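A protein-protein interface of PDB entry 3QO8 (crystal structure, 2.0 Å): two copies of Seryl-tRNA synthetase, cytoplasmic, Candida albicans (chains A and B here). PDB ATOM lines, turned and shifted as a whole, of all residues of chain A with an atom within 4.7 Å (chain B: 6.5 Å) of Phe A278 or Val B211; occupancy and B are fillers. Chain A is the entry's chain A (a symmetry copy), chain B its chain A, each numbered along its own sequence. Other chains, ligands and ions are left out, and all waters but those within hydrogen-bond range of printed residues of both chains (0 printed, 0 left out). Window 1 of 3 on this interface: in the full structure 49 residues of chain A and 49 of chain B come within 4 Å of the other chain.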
ATOM      1  N   VAL A 211       5.657   5.099  17.596  1.00  0.00           N
ATOM      2  CA  VAL A 211       5.787   4.182  16.462  1.00  0.00           C
ATOM      3  C   VAL A 211       5.381   2.755  16.790  1.00  0.00           C
ATOM      4  O   VAL A 211       5.483   1.861  15.938  1.00  0.00           O
ATOM      5  CB  VAL A 211       7.221   4.176  15.882  1.00  0.00           C
ATOM      6  CG1 VAL A 211       7.560   5.547  15.333  1.00  0.00           C
ATOM      7  CG2 VAL A 211       8.234   3.739  16.939  1.00  0.00           C
ATOM      8  N   GLU A 230       2.763  -6.082   5.565  1.00  0.00           N
ATOM      9  CA  GLU A 230       3.263  -4.734   5.818  1.00  0.00           C
ATOM     10  C   GLU A 230       3.872  -4.562   7.208  1.00  0.00           C
ATOM     11  O   GLU A 230       4.976  -4.029   7.331  1.00  0.00           O
ATOM     12  CB  GLU A 230       2.180  -3.672   5.567  1.00  0.00           C
ATOM     13  CG  GLU A 230       2.719  -2.241   5.442  1.00  0.00           C
ATOM     14  CD  GLU A 230       1.615  -1.176   5.414  1.00  0.00           C
ATOM     15  OE1 GLU A 230       0.616  -1.325   6.161  1.00  0.00           O
ATOM     16  OE2 GLU A 230       1.747  -0.188   4.651  1.00  0.00           O
ATOM     17  N   TYR A 232       5.465  -4.911  10.993  1.00  0.00           N
ATOM     18  CA  TYR A 232       6.370  -5.661  11.830  1.00  0.00           C
ATOM     19  C   TYR A 232       5.693  -5.845  13.166  1.00  0.00           C
ATOM     20  O   TYR A 232       5.142  -4.893  13.726  1.00  0.00           O
ATOM     21  CB  TYR A 232       7.656  -4.881  12.084  1.00  0.00           C
ATOM     22  CG  TYR A 232       8.612  -4.807  10.923  1.00  0.00           C
ATOM     23  CD1 TYR A 232       9.561  -5.798  10.718  1.00  0.00           C
ATOM     24  CD2 TYR A 232       8.579  -3.733  10.051  1.00  0.00           C
ATOM     25  CE1 TYR A 232      10.449  -5.729   9.668  1.00  0.00           C
ATOM     26  CE2 TYR A 232       9.464  -3.646   8.995  1.00  0.00           C
ATOM     27  CZ  TYR A 232      10.397  -4.646   8.812  1.00  0.00           C
ATOM     28  OH  TYR A 232      11.278  -4.559   7.765  1.00  0.00           O
ATOM     29  N   LEU A 243       4.728  -2.217  15.036  1.00  0.00           N
ATOM     30  CA  LEU A 243       5.321  -0.976  14.557  1.00  0.00           C
ATOM     31  C   LEU A 243       4.414  -0.359  13.494  1.00  0.00           C
ATOM     32  O   LEU A 243       3.833  -1.077  12.670  1.00  0.00           O
ATOM     33  CB  LEU A 243       6.706  -1.247  13.971  1.00  0.00           C
ATOM     34  CG  LEU A 243       7.781  -1.553  15.021  1.00  0.00           C
ATOM     35  CD1 LEU A 243       9.085  -1.916  14.317  1.00  0.00           C
ATOM     36  CD2 LEU A 243       7.981  -0.348  15.932  1.00  0.00           C
ATOM     37  N   ILE A 244       4.289   0.963  13.501  1.00  0.00           N
ATOM     38  CA  ILE A 244       3.400   1.638  12.558  1.00  0.00           C
ATOM     39  C   ILE A 244       4.018   1.737  11.168  1.00  0.00           C
ATOM     40  O   ILE A 244       5.234   1.838  11.041  1.00  0.00           O
ATOM     41  CB  ILE A 244       3.000   3.049  13.059  1.00  0.00           C
ATOM     42  CG1 ILE A 244       4.197   4.013  13.029  1.00  0.00           C
ATOM     43  CG2 ILE A 244       2.353   2.948  14.481  1.00  0.00           C
ATOM     44  CD1 ILE A 244       3.861   5.465  13.442  1.00  0.00           C
ATOM     45  N   ALA A 245       3.167   1.692  10.135  1.00  0.00           N
ATOM     46  CA  ALA A 245       3.585   1.878   8.749  1.00  0.00           C
ATOM     47  C   ALA A 245       3.526   3.349   8.359  1.00  0.00           C
ATOM     48  O   ALA A 245       4.119   3.764   7.364  1.00  0.00           O
ATOM     49  CB  ALA A 245       2.678   1.035   7.801  1.00  0.00           C
ATOM     50  N   SER A 276       8.786   8.085  12.387  1.00  0.00           N
ATOM     51  CA  SER A 276       9.363   7.059  11.531  1.00  0.00           C
ATOM     52  C   SER A 276       8.254   6.068  11.158  1.00  0.00           C
ATOM     53  O   SER A 276       7.219   5.998  11.838  1.00  0.00           O
ATOM     54  CB  SER A 276      10.528   6.356  12.221  1.00  0.00           C
ATOM     55  OG  SER A 276      11.647   7.231  12.255  1.00  0.00           O
ATOM     56  N   CYS A 277       8.482   5.331  10.073  1.00  0.00           N
ATOM     57  CA  CYS A 277       7.513   4.406   9.491  1.00  0.00           C
ATOM     58  C   CYS A 277       8.245   3.132   9.128  1.00  0.00           C
ATOM     59  O   CYS A 277       9.364   3.184   8.619  1.00  0.00           O
ATOM     60  CB  CYS A 277       6.886   5.014   8.226  1.00  0.00           C
ATOM     61  SG  CYS A 277       6.158   6.657   8.515  1.00  0.00           S
ATOM     62  N   PHE A 278       7.616   1.988   9.375  1.00  0.00           N
ATOM     63  CA  PHE A 278       8.283   0.697   9.189  1.00  0.00           C
ATOM     64  C   PHE A 278       7.419  -0.213   8.337  1.00  0.00           C
ATOM     65  O   PHE A 278       6.240  -0.412   8.638  1.00  0.00           O
ATOM     66  CB  PHE A 278       8.569   0.062  10.562  1.00  0.00           C
ATOM     67  CG  PHE A 278       9.353   0.968  11.474  1.00  0.00           C
ATOM     68  CD1 PHE A 278      10.739   0.947  11.471  1.00  0.00           C
ATOM     69  CD2 PHE A 278       8.697   1.887  12.287  1.00  0.00           C
ATOM     70  CE1 PHE A 278      11.463   1.820  12.289  1.00  0.00           C
ATOM     71  CE2 PHE A 278       9.410   2.752  13.096  1.00  0.00           C
ATOM     72  CZ  PHE A 278      10.790   2.710  13.104  1.00  0.00           C
ATOM     73  N   ARG A 279       7.998  -0.753   7.264  1.00  0.00           N
ATOM     74  CA  ARG A 279       7.243  -1.592   6.356  1.00  0.00           C
ATOM     75  C   ARG A 279       8.059  -2.798   5.915  1.00  0.00           C
ATOM     76  O   ARG A 279       9.195  -2.659   5.492  1.00  0.00           O
ATOM     77  CB  ARG A 279       6.805  -0.772   5.145  1.00  0.00           C
ATOM     78  CG  ARG A 279       6.005   0.453   5.531  1.00  0.00           C
ATOM     79  CD  ARG A 279       5.405   1.139   4.320  1.00  0.00           C
ATOM     80  NE  ARG A 279       4.681   2.334   4.730  1.00  0.00           N
ATOM     81  CZ  ARG A 279       3.801   2.978   3.969  1.00  0.00           C
ATOM     82  NH1 ARG A 279       3.516   2.533   2.738  1.00  0.00           N
ATOM     83  NH2 ARG A 279       3.196   4.064   4.450  1.00  0.00           N
ATOM     84  N   ARG A 280       7.470  -3.982   6.037  1.00  0.00           N
ATOM     85  CA  ARG A 280       8.134  -5.214   5.623  1.00  0.00           C
ATOM     86  C   ARG A 280       8.344  -5.282   4.112  1.00  0.00           C
ATOM     87  O   ARG A 280       9.277  -5.933   3.651  1.00  0.00           O
ATOM     88  CB  ARG A 280       7.345  -6.432   6.112  1.00  0.00           C
ATOM     89  CG  ARG A 280       7.312  -6.556   7.650  1.00  0.00           C
ATOM     90  CD  ARG A 280       6.713  -7.892   8.090  1.00  0.00           C
ATOM     91  NE  ARG A 280       7.332  -8.998   7.370  1.00  0.00           N
ATOM     92  CZ  ARG A 280       6.650  -9.913   6.683  1.00  0.00           C
ATOM     93  NH1 ARG A 280       5.323  -9.864   6.643  1.00  0.00           N
ATOM     94  NH2 ARG A 280       7.296 -10.877   6.043  1.00  0.00           N
ATOM     95  N   HIS A 296      12.844  -0.172   4.457  1.00  0.00           N
ATOM     96  CA  HIS A 296      12.000  -0.761   5.506  1.00  0.00           C
ATOM     97  C   HIS A 296      11.672   0.235   6.624  1.00  0.00           C
ATOM     98  O   HIS A 296      10.753   0.005   7.398  1.00  0.00           O
ATOM     99  CB  HIS A 296      12.669  -1.999   6.125  1.00  0.00           C
ATOM    100  CG  HIS A 296      12.759  -3.165   5.185  1.00  0.00           C
ATOM    101  ND1 HIS A 296      11.643  -3.807   4.686  1.00  0.00           N
ATOM    102  CD2 HIS A 296      13.830  -3.791   4.643  1.00  0.00           C
ATOM    103  CE1 HIS A 296      12.024  -4.775   3.868  1.00  0.00           C
ATOM    104  NE2 HIS A 296      13.344  -4.790   3.831  1.00  0.00           N
ATOM    105  N   ALA A 297      12.435   1.321   6.704  1.00  0.00           N
ATOM    106  CA  ALA A 297      12.263   2.342   7.750  1.00  0.00           C
ATOM    107  C   ALA A 297      12.508   3.695   7.117  1.00  0.00           C
ATOM    108  O   ALA A 297      13.502   3.878   6.411  1.00  0.00           O
ATOM    109  CB  ALA A 297      13.266   2.113   8.914  1.00  0.00           C
ATOM    110  N   ALA B 209      21.617   6.158  12.438  1.00  0.00           N
ATOM    111  CA  ALA B 209      21.703   4.706  12.465  1.00  0.00           C
ATOM    112  C   ALA B 209      20.335   4.079  12.271  1.00  0.00           C
ATOM    113  O   ALA B 209      19.324   4.649  12.688  1.00  0.00           O
ATOM    114  CB  ALA B 209      22.311   4.252  13.825  1.00  0.00           C
ATOM    115  N   PRO B 210      20.300   2.885  11.667  1.00  0.00           N
ATOM    116  CA  PRO B 210      19.040   2.139  11.589  1.00  0.00           C
ATOM    117  C   PRO B 210      18.647   1.692  12.994  1.00  0.00           C
ATOM    118  O   PRO B 210      19.524   1.513  13.837  1.00  0.00           O
ATOM    119  CB  PRO B 210      19.410   0.932  10.727  1.00  0.00           C
ATOM    120  CG  PRO B 210      20.885   0.754  10.950  1.00  0.00           C
ATOM    121  CD  PRO B 210      21.435   2.132  11.101  1.00  0.00           C
ATOM    122  N   VAL B 211      17.358   1.542  13.260  1.00  0.00           N
ATOM    123  CA  VAL B 211      16.915   1.172  14.606  1.00  0.00           C
ATOM    124  C   VAL B 211      16.614  -0.309  14.756  1.00  0.00           C
ATOM    125  O   VAL B 211      16.187  -0.758  15.830  1.00  0.00           O
ATOM    126  CB  VAL B 211      15.677   1.985  15.053  1.00  0.00           C
ATOM    127  CG1 VAL B 211      16.029   3.456  15.133  1.00  0.00           C
ATOM    128  CG2 VAL B 211      14.502   1.750  14.106  1.00  0.00           C
ATOM    129  N   MET B 212      16.824  -1.065  13.677  1.00  0.00           N
ATOM    130  CA  MET B 212      16.759  -2.522  13.731  1.00  0.00           C
ATOM    131  C   MET B 212      18.138  -3.106  13.468  1.00  0.00           C
ATOM    132  O   MET B 212      18.906  -2.567  12.667  1.00  0.00           O
ATOM    133  CB  MET B 212      15.803  -3.062  12.671  1.00  0.00           C
ATOM    134  CG  MET B 212      14.359  -2.730  12.932  1.00  0.00           C
ATOM    135  SD  MET B 212      13.289  -3.559  11.757  1.00  0.00           S
ATOM    136  CE  MET B 212      11.721  -2.781  12.159  1.00  0.00           C
ATOM    137  N   MET B 213      18.451  -4.208  14.137  1.00  0.00           N
ATOM    138  CA  MET B 213      19.727  -4.895  13.941  1.00  0.00           C
ATOM    139  C   MET B 213      19.503  -6.382  13.847  1.00  0.00           C
ATOM    140  O   MET B 213      18.624  -6.919  14.523  1.00  0.00           O
ATOM    141  CB  MET B 213      20.693  -4.622  15.094  1.00  0.00           C
ATOM    142  CG  MET B 213      21.428  -3.306  15.001  1.00  0.00           C
ATOM    143  SD  MET B 213      22.649  -3.127  16.324  1.00  0.00           S
ATOM    144  CE  MET B 213      23.971  -4.240  15.874  1.00  0.00           C
ATOM    145  N   VAL B 234      11.806  -7.976  17.106  1.00  0.00           N
ATOM    146  CA  VAL B 234      10.968  -7.649  15.965  1.00  0.00           C
ATOM    147  C   VAL B 234      10.698  -8.921  15.168  1.00  0.00           C
ATOM    148  O   VAL B 234      11.624  -9.661  14.870  1.00  0.00           O
ATOM    149  CB  VAL B 234      11.667  -6.602  15.065  1.00  0.00           C
ATOM    150  CG1 VAL B 234      10.914  -6.405  13.786  1.00  0.00           C
ATOM    151  CG2 VAL B 234      11.805  -5.273  15.809  1.00  0.00           C
ATOM    152  N   TYR B 242      16.251  -7.199  16.300  1.00  0.00           N
ATOM    153  CA  TYR B 242      16.034  -6.446  17.528  1.00  0.00           C
ATOM    154  C   TYR B 242      15.936  -4.957  17.226  1.00  0.00           C
ATOM    155  O   TYR B 242      16.607  -4.459  16.327  1.00  0.00           O
ATOM    156  CB  TYR B 242      17.179  -6.701  18.505  1.00  0.00           C
ATOM    157  CG  TYR B 242      17.150  -8.090  19.093  1.00  0.00           C
ATOM    158  CD1 TYR B 242      16.482  -8.345  20.280  1.00  0.00           C
ATOM    159  CD2 TYR B 242      17.766  -9.153  18.446  1.00  0.00           C
ATOM    160  CE1 TYR B 242      16.440  -9.616  20.818  1.00  0.00           C
ATOM    161  CE2 TYR B 242      17.728 -10.428  18.975  1.00  0.00           C
ATOM    162  CZ  TYR B 242      17.065 -10.656  20.160  1.00  0.00           C
ATOM    163  OH  TYR B 242      17.030 -11.927  20.690  1.00  0.00           O
ATOM    164  N   LEU B 243      15.102  -4.252  17.979  1.00  0.00           N
ATOM    165  CA  LEU B 243      15.163  -2.798  18.014  1.00  0.00           C
ATOM    166  C   LEU B 243      16.326  -2.362  18.903  1.00  0.00           C
ATOM    167  O   LEU B 243      16.584  -2.976  19.947  1.00  0.00           O
ATOM    168  CB  LEU B 243      13.851  -2.229  18.551  1.00  0.00           C
ATOM    169  CG  LEU B 243      12.678  -2.324  17.567  1.00  0.00           C
ATOM    170  CD1 LEU B 243      11.406  -1.832  18.250  1.00  0.00           C
ATOM    171  CD2 LEU B 243      12.972  -1.496  16.322  1.00  0.00           C
ATOM    172  N   ILE B 244      17.029  -1.308  18.505  1.00  0.00           N
ATOM    173  CA  ILE B 244      18.192  -0.852  19.262  1.00  0.00           C
ATOM    174  C   ILE B 244      17.789  -0.070  20.507  1.00  0.00           C
ATOM    175  O   ILE B 244      16.759   0.597  20.508  1.00  0.00           O
ATOM    176  CB  ILE B 244      19.143   0.004  18.387  1.00  0.00           C
ATOM    177  CG1 ILE B 244      18.510   1.361  18.035  1.00  0.00           C
ATOM    178  CG2 ILE B 244      19.570  -0.801  17.115  1.00  0.00           C
ATOM    179  CD1 ILE B 244      19.429   2.306  17.227  1.00  0.00           C
ATOM    180  N   ALA B 245      18.603  -0.176  21.565  1.00  0.00           N
ATOM    181  CA  ALA B 245      18.416   0.588  22.794  1.00  0.00           C
ATOM    182  C   ALA B 245      19.155   1.917  22.723  1.00  0.00           C
ATOM    183  O   ALA B 245      18.886   2.834  23.498  1.00  0.00           O
ATOM    184  CB  ALA B 245      18.918  -0.239  24.018  1.00  0.00           C
ATOM    185  N   PRO B 250      24.357  -0.067  16.850  1.00  0.00           N
ATOM    186  CA  PRO B 250      24.692  -0.232  15.425  1.00  0.00           C
ATOM    187  C   PRO B 250      25.966   0.525  15.014  1.00  0.00           C
ATOM    188  O   PRO B 250      26.715   0.057  14.162  1.00  0.00           O
ATOM    189  CB  PRO B 250      23.449   0.319  14.686  1.00  0.00           C
ATOM    190  CG  PRO B 250      22.774   1.261  15.674  1.00  0.00           C
ATOM    191  CD  PRO B 250      23.085   0.650  17.064  1.00  0.00           C
ATOM    192  N   SER B 275      19.530   8.502  16.554  1.00  0.00           N
ATOM    193  CA  SER B 275      18.522   7.487  16.294  1.00  0.00           C
ATOM    194  C   SER B 275      17.442   7.625  17.339  1.00  0.00           C
ATOM    195  O   SER B 275      17.654   8.253  18.378  1.00  0.00           O
ATOM    196  CB  SER B 275      19.135   6.088  16.400  1.00  0.00           C
ATOM    197  OG  SER B 275      19.404   5.761  17.771  1.00  0.00           O
ATOM    198  N   SER B 276      16.289   7.034  17.072  1.00  0.00           N
ATOM    199  CA  SER B 276      15.380   6.689  18.153  1.00  0.00           C
ATOM    200  C   SER B 276      15.952   5.472  18.890  1.00  0.00           C
ATOM    201  O   SER B 276      16.793   4.743  18.341  1.00  0.00           O
ATOM    202  CB  SER B 276      13.975   6.409  17.625  1.00  0.00           C
ATOM    203  OG  SER B 276      13.367   7.635  17.245  1.00  0.00           O
ATOM    204  N   CYS B 277      15.499   5.283  20.128  1.00  0.00           N
ATOM    205  CA  CYS B 277      15.991   4.247  21.033  1.00  0.00           C
ATOM    206  C   CYS B 277      14.795   3.614  21.710  1.00  0.00           C
ATOM    207  O   CYS B 277      13.859   4.312  22.095  1.00  0.00           O
ATOM    208  CB  CYS B 277      16.916   4.862  22.097  1.00  0.00           C
ATOM    209  SG  CYS B 277      18.278   5.832  21.377  1.00  0.00           S
ATOM    210  N   PHE B 278      14.827   2.295  21.869  1.00  0.00           N
ATOM    211  CA  PHE B 278      13.668   1.563  22.388  1.00  0.00           C
ATOM    212  C   PHE B 278      14.094   0.670  23.537  1.00  0.00           C
ATOM    213  O   PHE B 278      15.034  -0.116  23.399  1.00  0.00           O
ATOM    214  CB  PHE B 278      13.027   0.741  21.255  1.00  0.00           C
ATOM    215  CG  PHE B 278      12.667   1.577  20.056  1.00  0.00           C
ATOM    216  CD1 PHE B 278      11.422   2.180  19.963  1.00  0.00           C
ATOM    217  CD2 PHE B 278      13.602   1.810  19.054  1.00  0.00           C
ATOM    218  CE1 PHE B 278      11.107   2.991  18.868  1.00  0.00           C
ATOM    219  CE2 PHE B 278      13.294   2.611  17.970  1.00  0.00           C
ATOM    220  CZ  PHE B 278      12.046   3.191  17.873  1.00  0.00           C
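O of Val B211 is in hydrogen-bond range of N of Ile B244 (2.9 Å).
The backbone carbonyl oxygen (O) of Ile B244 lies within hydrogen-bond range of the backbone NH (N) of Phe B278.
O of Val A211 lies within hydrogen-bond range of N of Ile A244, 2.9 Å away.
O of Tyr A232 sits at hydrogen-bond distance from N of Leu A243 (3.0 Å).
OH of Tyr A232 lies within hydrogen-bond range of ND1 of His A296 (3.2 Å).
N of Phe A278 is in hydrogen-bond range of O of Ile A244, at 2.9 Å.
Among the printed residues, merely in contact across the chains: Tyr A232 with Val B234, Leu A243 with Met B212, Val A211 with Phe B278, Phe A278 with Val B211, Tyr A232 with Met B212 and Phe A278 with Met B212.
Of the printed residues of chain B, Tyr A232 touches Met B212 and Val B234.
Phe A278 touches two residues of chain B.
Printed residues of chain A within 4 Å of Val B211: Phe A278.
Printed residues of chain A within 4 Å of Met B212: Tyr A232 (3.9 Å), Leu A243 (3.5 Å) and Phe A278 (3.9 Å).
Of the printed residues of chain A, Val B234 touches Tyr A232 (3.4 Å).
Ala B245 touches none of the printed residues of chain A.
Of the printed residues of chain A, Phe B278 touches Val A211 (3.5 Å).
The nearest residue of chain B that does not touch Phe A278 is Phe B278 (5.0 Å).
The nearest printed residue of chain A that does not touch Val B211 is Ala A297 (5.3 Å).
Hydrophobic or aromatic side chains of chain A that line the printed part of chain B: Val A211, Tyr A232, Leu A243 and Phe A278.
Of the 15 printed residues of chain B, 4 touch a printed residue of chain A.
Printed residues of chain B that touch a printed residue of chain A: Val B211, Met B212, Val B234 and Phe B278.
Along chain B the printed residues that touch a printed residue of chain A span positions 211 to 278.
Among the printed residues, no Asp or Glu carboxylate lies within 4 Å of a Lys or Arg side-chain nitrogen of the other chain.
Val A211 touches Phe B278, and with the chains exchanged Phe A278 touches Val B211.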
